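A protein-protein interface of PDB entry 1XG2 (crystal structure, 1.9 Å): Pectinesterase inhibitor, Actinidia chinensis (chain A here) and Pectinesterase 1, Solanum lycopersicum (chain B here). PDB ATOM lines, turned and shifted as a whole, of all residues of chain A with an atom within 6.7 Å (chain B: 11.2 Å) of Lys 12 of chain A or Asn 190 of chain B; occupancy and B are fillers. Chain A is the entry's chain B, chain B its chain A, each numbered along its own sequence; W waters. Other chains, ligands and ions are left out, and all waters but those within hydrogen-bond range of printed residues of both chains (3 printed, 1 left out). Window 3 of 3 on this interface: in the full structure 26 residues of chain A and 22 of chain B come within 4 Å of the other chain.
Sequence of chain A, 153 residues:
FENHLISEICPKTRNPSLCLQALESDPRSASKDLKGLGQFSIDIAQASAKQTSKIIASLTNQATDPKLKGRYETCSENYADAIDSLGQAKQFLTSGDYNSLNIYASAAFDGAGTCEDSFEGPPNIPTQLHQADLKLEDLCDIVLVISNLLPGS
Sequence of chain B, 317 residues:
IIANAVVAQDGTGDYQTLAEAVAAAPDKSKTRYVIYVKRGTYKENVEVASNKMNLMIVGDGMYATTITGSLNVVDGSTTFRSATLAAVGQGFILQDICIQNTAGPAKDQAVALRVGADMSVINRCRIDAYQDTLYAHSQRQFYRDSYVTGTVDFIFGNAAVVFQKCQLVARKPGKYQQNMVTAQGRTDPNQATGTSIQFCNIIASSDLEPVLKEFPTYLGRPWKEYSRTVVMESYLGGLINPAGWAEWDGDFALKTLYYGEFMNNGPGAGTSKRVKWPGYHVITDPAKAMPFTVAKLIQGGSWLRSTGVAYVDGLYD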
ATOM      1  N   SER A   7      -9.301  14.088  15.769  1.00  0.00           N
ATOM      2  CA  SER A   7      -8.838  15.069  14.788  1.00  0.00           C
ATOM      3  C   SER A   7      -7.388  14.869  14.352  1.00  0.00           C
ATOM      4  O   SER A   7      -6.987  15.362  13.299  1.00  0.00           O
ATOM      5  CB  SER A   7      -9.035  16.502  15.306  1.00  0.00           C
ATOM      6  OG  SER A   7      -8.065  16.777  16.302  1.00  0.00           O
ATOM      7  N   GLU A   8      -6.608  14.146  15.152  1.00  0.00           N
ATOM      8  CA  GLU A   8      -5.249  13.774  14.757  1.00  0.00           C
ATOM      9  C   GLU A   8      -5.151  12.456  14.014  1.00  0.00           C
ATOM     10  O   GLU A   8      -4.153  12.203  13.333  1.00  0.00           O
ATOM     11  CB  GLU A   8      -4.355  13.679  15.988  1.00  0.00           C
ATOM     12  CG  GLU A   8      -4.227  14.980  16.752  1.00  0.00           C
ATOM     13  CD  GLU A   8      -3.210  14.859  17.869  1.00  0.00           C
ATOM     14  OE1 GLU A   8      -3.523  15.251  18.997  1.00  0.00           O
ATOM     15  OE2 GLU A   8      -2.110  14.344  17.597  1.00  0.00           O
ATOM     16  N   ILE A   9      -6.156  11.600  14.176  1.00  0.00           N
ATOM     17  CA  ILE A   9      -6.117  10.256  13.609  1.00  0.00           C
ATOM     18  C   ILE A   9      -6.764  10.219  12.240  1.00  0.00           C
ATOM     19  O   ILE A   9      -6.113   9.919  11.248  1.00  0.00           O
ATOM     20  CB  ILE A   9      -6.806   9.250  14.557  1.00  0.00           C
ATOM     21  CG1 ILE A   9      -6.042   9.151  15.878  1.00  0.00           C
ATOM     22  CG2 ILE A   9      -6.848   7.868  13.925  1.00  0.00           C
ATOM     23  CD1 ILE A   9      -6.852   8.477  16.992  1.00  0.00           C
ATOM     24  N   CYS A  10      -8.054  10.537  12.185  1.00  0.00           N
ATOM     25  CA  CYS A  10      -8.820  10.313  10.967  1.00  0.00           C
ATOM     26  C   CYS A  10      -8.267  11.017   9.714  1.00  0.00           C
ATOM     27  O   CYS A  10      -8.167  10.381   8.675  1.00  0.00           O
ATOM     28  CB  CYS A  10     -10.310  10.593  11.206  1.00  0.00           C
ATOM     29  SG  CYS A  10     -10.959   9.306  12.292  1.00  0.00           S
ATOM     30  N   PRO A  11      -7.890  12.290   9.792  1.00  0.00           N
ATOM     31  CA  PRO A  11      -7.293  12.975   8.620  1.00  0.00           C
ATOM     32  C   PRO A  11      -6.012  12.345   8.043  1.00  0.00           C
ATOM     33  O   PRO A  11      -5.723  12.561   6.869  1.00  0.00           O
ATOM     34  CB  PRO A  11      -6.986  14.381   9.138  1.00  0.00           C
ATOM     35  CG  PRO A  11      -7.853  14.554  10.322  1.00  0.00           C
ATOM     36  CD  PRO A  11      -8.040  13.194  10.946  1.00  0.00           C
ATOM     37  N   LYS A  12      -5.274  11.590   8.853  1.00  0.00           N
ATOM     38  CA  LYS A  12      -4.055  10.907   8.405  1.00  0.00           C
ATOM     39  C   LYS A  12      -4.311   9.531   7.789  1.00  0.00           C
ATOM     40  O   LYS A  12      -3.380   8.915   7.270  1.00  0.00           O
ATOM     41  CB  LYS A  12      -3.074  10.754   9.576  1.00  0.00           C
ATOM     42  CG  LYS A  12      -2.374  12.032   9.998  1.00  0.00           C
ATOM     43  CD  LYS A  12      -1.555  11.806  11.277  1.00  0.00           C
ATOM     44  CE  LYS A  12      -1.066  13.113  11.884  1.00  0.00           C
ATOM     45  NZ  LYS A  12      -2.135  13.855  12.625  1.00  0.00           N
ATOM     46  N   THR A  13      -5.536   9.015   7.879  1.00  0.00           N
ATOM     47  CA  THR A  13      -5.841   7.719   7.293  1.00  0.00           C
ATOM     48  C   THR A  13      -6.247   7.879   5.838  1.00  0.00           C
ATOM     49  O   THR A  13      -6.608   8.964   5.389  1.00  0.00           O
ATOM     50  CB  THR A  13      -7.011   6.979   8.040  1.00  0.00           C
ATOM     51  OG1 THR A  13      -8.249   7.691   7.864  1.00  0.00           O
ATOM     52  CG2 THR A  13      -6.793   6.932   9.542  1.00  0.00           C
ATOM     53  N   ARG A  14      -6.244   6.772   5.117  1.00  0.00           N
ATOM     54  CA  ARG A  14      -6.613   6.797   3.714  1.00  0.00           C
ATOM     55  C   ARG A  14      -8.123   6.891   3.491  1.00  0.00           C
ATOM     56  O   ARG A  14      -8.565   7.238   2.393  1.00  0.00           O
ATOM     57  CB  ARG A  14      -6.010   5.596   2.983  1.00  0.00           C
ATOM     58  CG  ARG A  14      -6.493   4.281   3.461  1.00  0.00           C
ATOM     59  CD  ARG A  14      -5.504   3.149   3.214  1.00  0.00           C
ATOM     60  NE  ARG A  14      -5.731   2.502   1.925  1.00  0.00           N
ATOM     61  CZ  ARG A  14      -4.815   2.335   0.976  1.00  0.00           C
ATOM     62  NH1 ARG A  14      -3.587   2.817   1.093  1.00  0.00           N
ATOM     63  NH2 ARG A  14      -5.136   1.696  -0.125  1.00  0.00           N
ATOM     64  N   ASN A  15      -8.917   6.604   4.521  1.00  0.00           N
ATOM     65  CA  ASN A  15     -10.366   6.781   4.447  1.00  0.00           C
ATOM     66  C   ASN A  15     -10.863   7.464   5.731  1.00  0.00           C
ATOM     67  O   ASN A  15     -11.335   6.799   6.657  1.00  0.00           O
ATOM     68  CB  ASN A  15     -11.070   5.431   4.238  1.00  0.00           C
ATOM     69  CG  ASN A  15     -12.534   5.581   3.906  1.00  0.00           C
ATOM     70  OD1 ASN A  15     -13.130   6.640   4.141  1.00  0.00           O
ATOM     71  ND2 ASN A  15     -13.135   4.517   3.357  1.00  0.00           N
ATOM     72  N   PRO A  16     -10.719   8.785   5.807  1.00  0.00           N
ATOM     73  CA  PRO A  16     -11.177   9.531   6.988  1.00  0.00           C
ATOM     74  C   PRO A  16     -12.657   9.353   7.320  1.00  0.00           C
ATOM     75  O   PRO A  16     -13.018   9.399   8.485  1.00  0.00           O
ATOM     76  CB  PRO A  16     -10.873  10.996   6.611  1.00  0.00           C
ATOM     77  CG  PRO A  16      -9.764  10.901   5.638  1.00  0.00           C
ATOM     78  CD  PRO A  16     -10.063   9.668   4.819  1.00  0.00           C
ATOM     79  N   ASN A 102       3.261  -1.443  14.797  1.00  0.00           N
ATOM     80  CA  ASN A 102       3.225  -0.961  13.411  1.00  0.00           C
ATOM     81  C   ASN A 102       3.487  -2.108  12.422  1.00  0.00           C
ATOM     82  O   ASN A 102       2.697  -2.352  11.519  1.00  0.00           O
ATOM     83  CB  ASN A 102       4.211   0.187  13.196  1.00  0.00           C
ATOM     84  CG  ASN A 102       4.072   0.807  11.838  1.00  0.00           C
ATOM     85  OD1 ASN A 102       4.331   0.171  10.795  1.00  0.00           O
ATOM     86  ND2 ASN A 102       3.677   2.056  11.827  1.00  0.00           N
ATOM     87  N   SER A 106       0.950  -3.453   9.725  1.00  0.00           N
ATOM     88  CA  SER A 106       1.377  -3.354   8.335  1.00  0.00           C
ATOM     89  C   SER A 106       1.228  -4.694   7.625  1.00  0.00           C
ATOM     90  O   SER A 106       0.796  -4.745   6.468  1.00  0.00           O
ATOM     91  CB  SER A 106       2.833  -2.878   8.225  1.00  0.00           C
ATOM     92  OG  SER A 106       2.971  -1.529   8.607  1.00  0.00           O
ATOM     93  N   ASP A 141      -5.232   0.869   8.578  1.00  0.00           N
ATOM     94  CA  ASP A 141      -4.589   2.172   8.514  1.00  0.00           C
ATOM     95  C   ASP A 141      -4.897   3.026   9.757  1.00  0.00           C
ATOM     96  O   ASP A 141      -4.051   3.798  10.197  1.00  0.00           O
ATOM     97  CB  ASP A 141      -4.992   2.897   7.245  1.00  0.00           C
ATOM     98  CG  ASP A 141      -4.009   3.962   6.858  1.00  0.00           C
ATOM     99  OD1 ASP A 141      -2.781   3.756   7.010  1.00  0.00           O
ATOM    100  OD2 ASP A 141      -4.368   5.031   6.366  1.00  0.00           O
ATOM    101  N   ILE A 142      -6.084   2.874  10.340  1.00  0.00           N
ATOM    102  CA  ILE A 142      -6.390   3.553  11.595  1.00  0.00           C
ATOM    103  C   ILE A 142      -5.388   3.088  12.657  1.00  0.00           C
ATOM    104  O   ILE A 142      -4.836   3.882  13.404  1.00  0.00           O
ATOM    105  CB  ILE A 142      -7.848   3.303  12.072  1.00  0.00           C
ATOM    106  CG1 ILE A 142      -8.873   3.754  11.030  1.00  0.00           C
ATOM    107  CG2 ILE A 142      -8.126   4.104  13.330  1.00  0.00           C
ATOM    108  CD1 ILE A 142     -10.263   3.215  11.281  1.00  0.00           C
ATOM    109  N   LEU A 144      -2.410   1.795  12.159  1.00  0.00           N
ATOM    110  CA  LEU A 144      -1.076   2.278  11.815  1.00  0.00           C
ATOM    111  C   LEU A 144      -0.890   3.734  12.251  1.00  0.00           C
ATOM    112  O   LEU A 144       0.143   4.095  12.799  1.00  0.00           O
ATOM    113  CB  LEU A 144      -0.824   2.140  10.307  1.00  0.00           C
ATOM    114  CG  LEU A 144      -0.699   0.707   9.791  1.00  0.00           C
ATOM    115  CD1 LEU A 144      -0.759   0.646   8.270  1.00  0.00           C
ATOM    116  CD2 LEU A 144       0.623   0.086  10.275  1.00  0.00           C
ATOM    117  N   VAL A 145      -1.903   4.570  12.023  1.00  0.00           N
ATOM    118  CA  VAL A 145      -1.800   5.985  12.369  1.00  0.00           C
ATOM    119  C   VAL A 145      -1.648   6.133  13.887  1.00  0.00           C
ATOM    120  O   VAL A 145      -0.810   6.894  14.381  1.00  0.00           O
ATOM    121  CB  VAL A 145      -3.009   6.777  11.847  1.00  0.00           C
ATOM    122  CG1 VAL A 145      -3.076   8.183  12.499  1.00  0.00           C
ATOM    123  CG2 VAL A 145      -2.928   6.905  10.348  1.00  0.00           C
ATOM    124  N   SER A 147      -0.470   3.900  15.927  1.00  0.00           N
ATOM    125  CA  SER A 147       0.861   3.383  16.308  1.00  0.00           C
ATOM    126  C   SER A 147       1.962   4.441  16.119  1.00  0.00           C
ATOM    127  O   SER A 147       2.965   4.431  16.851  1.00  0.00           O
ATOM    128  CB  SER A 147       1.226   2.094  15.544  1.00  0.00           C
ATOM    129  OG  SER A 147       1.654   2.367  14.204  1.00  0.00           O
ATOM    130  N   ASN A 148       1.796   5.336  15.147  1.00  0.00           N
ATOM    131  CA  ASN A 148       2.789   6.383  14.916  1.00  0.00           C
ATOM    132  C   ASN A 148       2.595   7.602  15.822  1.00  0.00           C
ATOM    133  O   ASN A 148       3.545   8.322  16.073  1.00  0.00           O
ATOM    134  CB  ASN A 148       2.830   6.819  13.446  1.00  0.00           C
ATOM    135  CG  ASN A 148       3.213   5.679  12.498  1.00  0.00           C
ATOM    136  OD1 ASN A 148       3.911   4.732  12.890  1.00  0.00           O
ATOM    137  ND2 ASN A 148       2.754   5.758  11.266  1.00  0.00           N
ATOM    138  N   LEU A 149       1.378   7.828  16.300  1.00  0.00           N
ATOM    139  CA  LEU A 149       1.105   8.916  17.241  1.00  0.00           C
ATOM    140  C   LEU A 149       1.534   8.578  18.678  1.00  0.00           C
ATOM    141  O   LEU A 149       1.839   9.478  19.461  1.00  0.00           O
ATOM    142  CB  LEU A 149      -0.379   9.274  17.249  1.00  0.00           C
ATOM    143  CG  LEU A 149      -0.956   9.895  15.983  1.00  0.00           C
ATOM    144  CD1 LEU A 149      -2.469   9.983  16.126  1.00  0.00           C
ATOM    145  CD2 LEU A 149      -0.342  11.264  15.719  1.00  0.00           C
ATOM    146  N   ASN B 158       6.908  -6.247   1.051  1.00  0.00           N
ATOM    147  CA  ASN B 158       6.773  -5.115   1.947  1.00  0.00           C
ATOM    148  C   ASN B 158       7.186  -5.461   3.370  1.00  0.00           C
ATOM    149  O   ASN B 158       6.602  -4.966   4.335  1.00  0.00           O
ATOM    150  CB  ASN B 158       5.338  -4.601   1.907  1.00  0.00           C
ATOM    151  CG  ASN B 158       5.168  -3.249   2.559  1.00  0.00           C
ATOM    152  OD1 ASN B 158       6.087  -2.401   2.502  1.00  0.00           O
ATOM    153  ND2 ASN B 158       4.031  -3.028   3.204  1.00  0.00           N
ATOM    154  N   ALA B 160       9.848  -5.188   6.562  1.00  0.00           N
ATOM    155  CA  ALA B 160      10.927  -4.332   7.022  1.00  0.00           C
ATOM    156  C   ALA B 160      12.137  -5.261   7.036  1.00  0.00           C
ATOM    157  O   ALA B 160      12.196  -6.203   7.831  1.00  0.00           O
ATOM    158  CB  ALA B 160      10.644  -3.786   8.390  1.00  0.00           C
ATOM    159  N   GLN B 184      10.009  -2.825  -4.310  1.00  0.00           N
ATOM    160  CA  GLN B 184       9.522  -2.676  -2.939  1.00  0.00           C
ATOM    161  C   GLN B 184       8.070  -2.198  -2.997  1.00  0.00           C
ATOM    162  O   GLN B 184       7.761  -1.256  -3.701  1.00  0.00           O
ATOM    163  CB  GLN B 184      10.417  -1.700  -2.176  1.00  0.00           C
ATOM    164  CG  GLN B 184      10.471  -1.947  -0.669  1.00  0.00           C
ATOM    165  CD  GLN B 184       9.183  -1.563   0.036  1.00  0.00           C
ATOM    166  OE1 GLN B 184       8.777  -2.208   1.026  1.00  0.00           O
ATOM    167  NE2 GLN B 184       8.529  -0.531  -0.464  1.00  0.00           N
ATOM    168  N   GLY B 185       7.202  -2.850  -2.240  1.00  0.00           N
ATOM    169  CA  GLY B 185       5.767  -2.688  -2.369  1.00  0.00           C
ATOM    170  C   GLY B 185       5.055  -2.045  -1.184  1.00  0.00           C
ATOM    171  O   GLY B 185       3.961  -2.493  -0.824  1.00  0.00           O
ATOM    172  N   ARG B 186       5.647  -1.017  -0.576  1.00  0.00           N
ATOM    173  CA  ARG B 186       4.969  -0.251   0.471  1.00  0.00           C
ATOM    174  C   ARG B 186       3.890   0.639  -0.142  1.00  0.00           C
ATOM    175  O   ARG B 186       4.178   1.521  -0.944  1.00  0.00           O
ATOM    176  CB  ARG B 186       5.943   0.614   1.286  1.00  0.00           C
ATOM    177  CG  ARG B 186       5.266   1.325   2.461  1.00  0.00           C
ATOM    178  CD  ARG B 186       6.199   2.070   3.393  1.00  0.00           C
ATOM    179  NE  ARG B 186       6.613   3.343   2.803  1.00  0.00           N
ATOM    180  CZ  ARG B 186       6.910   4.456   3.470  1.00  0.00           C
ATOM    181  NH1 ARG B 186       6.873   4.501   4.791  1.00  0.00           N
ATOM    182  NH2 ARG B 186       7.248   5.554   2.798  1.00  0.00           N
ATOM    183  N   THR B 187       2.654   0.393   0.274  1.00  0.00           N
ATOM    184  CA  THR B 187       1.465   0.996  -0.299  1.00  0.00           C
ATOM    185  C   THR B 187       1.073   2.273   0.441  1.00  0.00           C
ATOM    186  O   THR B 187       0.390   3.134  -0.106  1.00  0.00           O
ATOM    187  CB  THR B 187       0.328  -0.048  -0.201  1.00  0.00           C
ATOM    188  OG1 THR B 187       0.588  -1.112  -1.137  1.00  0.00           O
ATOM    189  CG2 THR B 187      -0.999   0.515  -0.630  1.00  0.00           C
ATOM    190  N   ASP B 188       1.525   2.385   1.679  1.00  0.00           N
ATOM    191  CA  ASP B 188       0.942   3.296   2.647  1.00  0.00           C
ATOM    192  C   ASP B 188       2.089   3.891   3.476  1.00  0.00           C
ATOM    193  O   ASP B 188       2.901   3.163   4.017  1.00  0.00           O
ATOM    194  CB  ASP B 188      -0.035   2.456   3.471  1.00  0.00           C
ATOM    195  CG  ASP B 188      -0.708   3.195   4.614  1.00  0.00           C
ATOM    196  OD1 ASP B 188      -0.331   4.313   5.012  1.00  0.00           O
ATOM    197  OD2 ASP B 188      -1.669   2.650   5.193  1.00  0.00           O
ATOM    198  N   PRO B 189       2.168   5.218   3.548  1.00  0.00           N
ATOM    199  CA  PRO B 189       3.273   5.892   4.219  1.00  0.00           C
ATOM    200  C   PRO B 189       3.264   5.757   5.747  1.00  0.00           C
ATOM    201  O   PRO B 189       4.247   6.125   6.371  1.00  0.00           O
ATOM    202  CB  PRO B 189       3.075   7.343   3.810  1.00  0.00           C
ATOM    203  CG  PRO B 189       1.661   7.477   3.594  1.00  0.00           C
ATOM    204  CD  PRO B 189       1.207   6.184   2.997  1.00  0.00           C
ATOM    205  N   ASN B 190       2.177   5.240   6.324  1.00  0.00           N
ATOM    206  CA  ASN B 190       2.099   4.983   7.750  1.00  0.00           C
ATOM    207  C   ASN B 190       2.748   3.642   8.128  1.00  0.00           C
ATOM    208  O   ASN B 190       2.937   3.356   9.308  1.00  0.00           O
ATOM    209  CB  ASN B 190       0.642   5.009   8.248  1.00  0.00           C
ATOM    210  CG  ASN B 190      -0.102   6.297   7.873  1.00  0.00           C
ATOM    211  OD1 ASN B 190      -1.209   6.255   7.315  1.00  0.00           O
ATOM    212  ND2 ASN B 190       0.491   7.430   8.185  1.00  0.00           N
ATOM    213  N   GLN B 191       3.077   2.829   7.128  1.00  0.00           N
ATOM    214  CA  GLN B 191       3.739   1.551   7.337  1.00  0.00           C
ATOM    215  C   GLN B 191       5.249   1.750   7.536  1.00  0.00           C
ATOM    216  O   GLN B 191       5.902   2.391   6.719  1.00  0.00           O
ATOM    217  CB  GLN B 191       3.496   0.602   6.148  1.00  0.00           C
ATOM    218  CG  GLN B 191       2.056   0.141   5.923  1.00  0.00           C
ATOM    219  CD  GLN B 191       1.920  -0.765   4.688  1.00  0.00           C
ATOM    220  OE1 GLN B 191       2.216  -0.351   3.555  1.00  0.00           O
ATOM    221  NE2 GLN B 191       1.487  -1.990   4.905  1.00  0.00           N
ATOM    222  N   ALA B 192       5.795   1.189   8.611  1.00  0.00           N
ATOM    223  CA  ALA B 192       7.239   1.294   8.890  1.00  0.00           C
ATOM    224  C   ALA B 192       8.016   0.145   8.233  1.00  0.00           C
ATOM    225  O   ALA B 192       8.713  -0.652   8.891  1.00  0.00           O
ATOM    226  CB  ALA B 192       7.503   1.341  10.366  1.00  0.00           C
ATOM    227  N   THR B 193       7.914   0.083   6.917  1.00  0.00           N
ATOM    228  CA  THR B 193       8.516  -0.991   6.150  1.00  0.00           C
ATOM    229  C   THR B 193       9.428  -0.414   5.097  1.00  0.00           C
ATOM    230  O   THR B 193       9.435   0.794   4.847  1.00  0.00           O
ATOM    231  CB  THR B 193       7.434  -1.822   5.488  1.00  0.00           C
ATOM    232  OG1 THR B 193       6.572  -0.962   4.734  1.00  0.00           O
ATOM    233  CG2 THR B 193       6.528  -2.457   6.528  1.00  0.00           C
ATOM    234  N   GLY B 194      10.172  -1.301   4.456  1.00  0.00           N
ATOM    235  CA  GLY B 194      11.084  -0.928   3.397  1.00  0.00           C
ATOM    236  C   GLY B 194      12.233  -1.896   3.293  1.00  0.00           C
ATOM    237  O   GLY B 194      12.437  -2.735   4.158  1.00  0.00           O
ATOM    238  N   GLU B 225       3.002   2.648  -4.415  1.00  0.00           N
ATOM    239  CA  GLU B 225       3.064   4.106  -4.476  1.00  0.00           C
ATOM    240  C   GLU B 225       4.099   4.715  -3.527  1.00  0.00           C
ATOM    241  O   GLU B 225       4.739   5.730  -3.852  1.00  0.00           O
ATOM    242  CB  GLU B 225       1.676   4.673  -4.177  1.00  0.00           C
ATOM    243  CG  GLU B 225       1.488   6.126  -4.570  1.00  0.00           C
ATOM    244  CD  GLU B 225       0.089   6.652  -4.234  1.00  0.00           C
ATOM    245  OE1 GLU B 225      -0.156   7.858  -4.434  1.00  0.00           O
ATOM    246  OE2 GLU B 225      -0.760   5.857  -3.772  1.00  0.00           O
ATOM    247  N   TYR B 226       4.251   4.092  -2.359  1.00  0.00           N
ATOM    248  CA  TYR B 226       5.227   4.519  -1.368  1.00  0.00           C
ATOM    249  C   TYR B 226       6.420   3.568  -1.233  1.00  0.00           C
ATOM    250  O   TYR B 226       6.964   3.394  -0.139  1.00  0.00           O
ATOM    251  CB  TYR B 226       4.522   4.749  -0.037  1.00  0.00           C
ATOM    252  CG  TYR B 226       3.598   5.941  -0.128  1.00  0.00           C
ATOM    253  CD1 TYR B 226       2.316   5.815  -0.637  1.00  0.00           C
ATOM    254  CD2 TYR B 226       4.036   7.204   0.233  1.00  0.00           C
ATOM    255  CE1 TYR B 226       1.467   6.939  -0.750  1.00  0.00           C
ATOM    256  CE2 TYR B 226       3.202   8.316   0.130  1.00  0.00           C
ATOM    257  CZ  TYR B 226       1.927   8.173  -0.362  1.00  0.00           C
ATOM    258  OH  TYR B 226       1.112   9.277  -0.463  1.00  0.00           O
ATOM    259  N   SER B 227       6.849   3.006  -2.367  1.00  0.00           N
ATOM    260  CA  SER B 227       8.032   2.151  -2.457  1.00  0.00           C
ATOM    261  C   SER B 227       9.182   2.809  -1.710  1.00  0.00           C
ATOM    262  O   SER B 227       9.420   4.001  -1.864  1.00  0.00           O
ATOM    263  CB  SER B 227       8.424   1.929  -3.929  1.00  0.00           C
ATOM    264  OG  SER B 227       9.351   0.876  -4.088  1.00  0.00           O
ATOM    265  N   ARG B 228       9.880   2.045  -0.883  1.00  0.00           N
ATOM    266  CA  ARG B 228      10.936   2.605  -0.053  1.00  0.00           C
ATOM    267  C   ARG B 228      12.126   1.662   0.039  1.00  0.00           C
ATOM    268  O   ARG B 228      12.042   0.606   0.654  1.00  0.00           O
ATOM    269  CB  ARG B 228      10.418   2.938   1.337  1.00  0.00           C
ATOM    270  CG  ARG B 228      11.476   3.552   2.233  1.00  0.00           C
ATOM    271  CD  ARG B 228      10.933   4.446   3.306  1.00  0.00           C
ATOM    272  NE  ARG B 228      10.357   3.640   4.365  1.00  0.00           N
ATOM    273  CZ  ARG B 228      10.440   3.914   5.656  1.00  0.00           C
ATOM    274  NH1 ARG B 228      11.047   5.012   6.084  1.00  0.00           N
ATOM    275  NH2 ARG B 228       9.887   3.090   6.537  1.00  0.00           N
ATOM    276  N   THR B 256       6.280  10.084  -4.519  1.00  0.00           N
ATOM    277  CA  THR B 256       5.942   9.523  -3.200  1.00  0.00           C
ATOM    278  C   THR B 256       6.849   8.367  -2.749  1.00  0.00           C
ATOM    279  O   THR B 256       6.901   8.048  -1.561  1.00  0.00           O
ATOM    280  CB  THR B 256       4.481   9.047  -3.188  1.00  0.00           C
ATOM    281  OG1 THR B 256       4.209   8.264  -4.363  1.00  0.00           O
ATOM    282  CG2 THR B 256       3.508  10.239  -3.272  1.00  0.00           C
ATOM    283  N   LEU B 297      15.383   0.064  11.528  1.00  0.00           N
ATOM    284  CA  LEU B 297      14.376  -0.448  10.595  1.00  0.00           C
ATOM    285  C   LEU B 297      13.735  -1.750  11.077  1.00  0.00           C
ATOM    286  O   LEU B 297      12.541  -1.955  10.900  1.00  0.00           O
ATOM    287  CB  LEU B 297      14.967  -0.629   9.197  1.00  0.00           C
ATOM    288  CG  LEU B 297      13.994  -1.103   8.101  1.00  0.00           C
ATOM    289  CD1 LEU B 297      12.906  -0.073   7.834  1.00  0.00           C
ATOM    290  CD2 LEU B 297      14.756  -1.395   6.828  1.00  0.00           C
HETATM  291  O   HOH W   1       1.222   8.067  10.597  1.00  0.00           O
HETATM  292  O   HOH W   2      -0.632   9.552   6.878  1.00  0.00           O
HETATM  293  O   HOH W   3      -2.142   4.886   2.080  1.00  0.00           O
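Printed residues of chain B that touch a printed residue of chain A: Thr 187, Asp 188, Asn 190, Gln 191 and Ala 192. Printed residues of chain A that touch a printed residue of chain B: Lys 12, Arg 14, Asn 102, Ser 106, Asp 141, Leu 144, Val 145 and Asn 148. Hydrophobic or aromatic side chains of chain A that line the printed part of chain B: Leu 144 and Val 145. Along chain A the printed residues that touch a printed residue of chain B span positions 12 to 148. Among the printed residues, no Asp or Glu carboxylate lies within 4 Å of a Lys or Arg side-chain nitrogen of the other chain.
Among the printed residues, merely in contact across the chains: Arg 14 of chain A with Thr 187 of chain B (3.9 Å), Asn 102 of chain A with Gln 191 of chain B (3.7 Å), Ser 106 of chain A with Ala 192 of chain B (3.9 Å), Leu 144 of chain A with Asp 188 of chain B (3.8 Å), Leu 144 of chain A with Asn 190 of chain B (3.8 Å), Leu 144 of chain A with Gln 191 of chain B (3.7 Å) and Val 145 of chain A with Asn 190 of chain B (3.5 Å).
Ile 9 of chain A touches none of the printed residues of chain B. No residue of chain B comes within 4 Å of Pro 11 of chain A. Of the printed residues of chain B, Asn 102 of chain A touches Asn 190, Gln 191 and Ala 192. Of chain B, only Asp 188 (2.4 Å) and Asn 190 (3.0 Å) come within 4 Å of Asp 141 of chain A. Of chain B, only Asn 190 (3.5 Å) comes within 4 Å of Val 145 of chain A. Asn 190 of chain B touches just these residues of chain A: Lys 12, Asn 102, Asp 141, Leu 144, Val 145 and Asn 148. Printed residues of chain A within 4 Å of Gln 191 of chain B: Asn 102, Ser 106 and Leu 144. Of the printed residues of chain A, Ala 192 of chain B touches Asn 102 (2.8 Å) and Ser 106 (3.9 Å). The nearest residue of chain B that does not touch Lys 12 of chain A is Asp 188 of chain B (6.0 Å). The nearest residue of chain A that does not touch Asn 190 of chain B is Thr 13 of chain A (4.9 Å).
Water W1 bridges the side-chain amide nitrogen of Asn 190 of chain B (2.6 Å) and the side-chain amide nitrogen of Asn 148 of chain A (2.9 Å). Water W3 bridges NH1 of Arg 14 of chain A (2.7 Å) and OD1 of Asp 188 of chain B (3.5 Å). Water W2 bridges ND2 of Asn 190 of chain B (2.7 Å) and O of Lys 12 of chain A (2.8 Å).
The side-chain amide oxygen (OD1) of Asn 190 of chain B sits close to the side-chain carboxylate (OD1) of Asp 141 of chain A, 3.0 Å away. O of Ser 106 of chain A is in hydrogen-bond range of NE2 of Gln 191 of chain B. The backbone carbonyl oxygen of Asn 190 of chain B is in hydrogen-bond range of the side-chain amide nitrogen of Asn 102 of chain A (2.9 Å). OD1 of Asn 102 of chain A is in hydrogen-bond range of N of Ala 192 of chain B, 2.8 Å away. The side-chain carboxylate (OD2) of Asp 188 of chain B sits close to the side-chain carboxylate (OD1) of Asp 141 of chain A. OD1 of Asn 190 of chain B sits close to O of Lys 12 of chain A (3.4 Å). O of Asn 190 of chain B lies within hydrogen-bond range of ND2 of Asn 148 of chain A, 3.1 Å away.
O of Asn 102 of chain A is in hydrogen-bond range of OG of Ser 106 of chain A, at 3.0 Å. The side-chain hydroxyl of Ser 147 of chain A sits at hydrogen-bond distance from the side-chain amide nitrogen of Asn 102 of chain A, 3.1 Å away.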
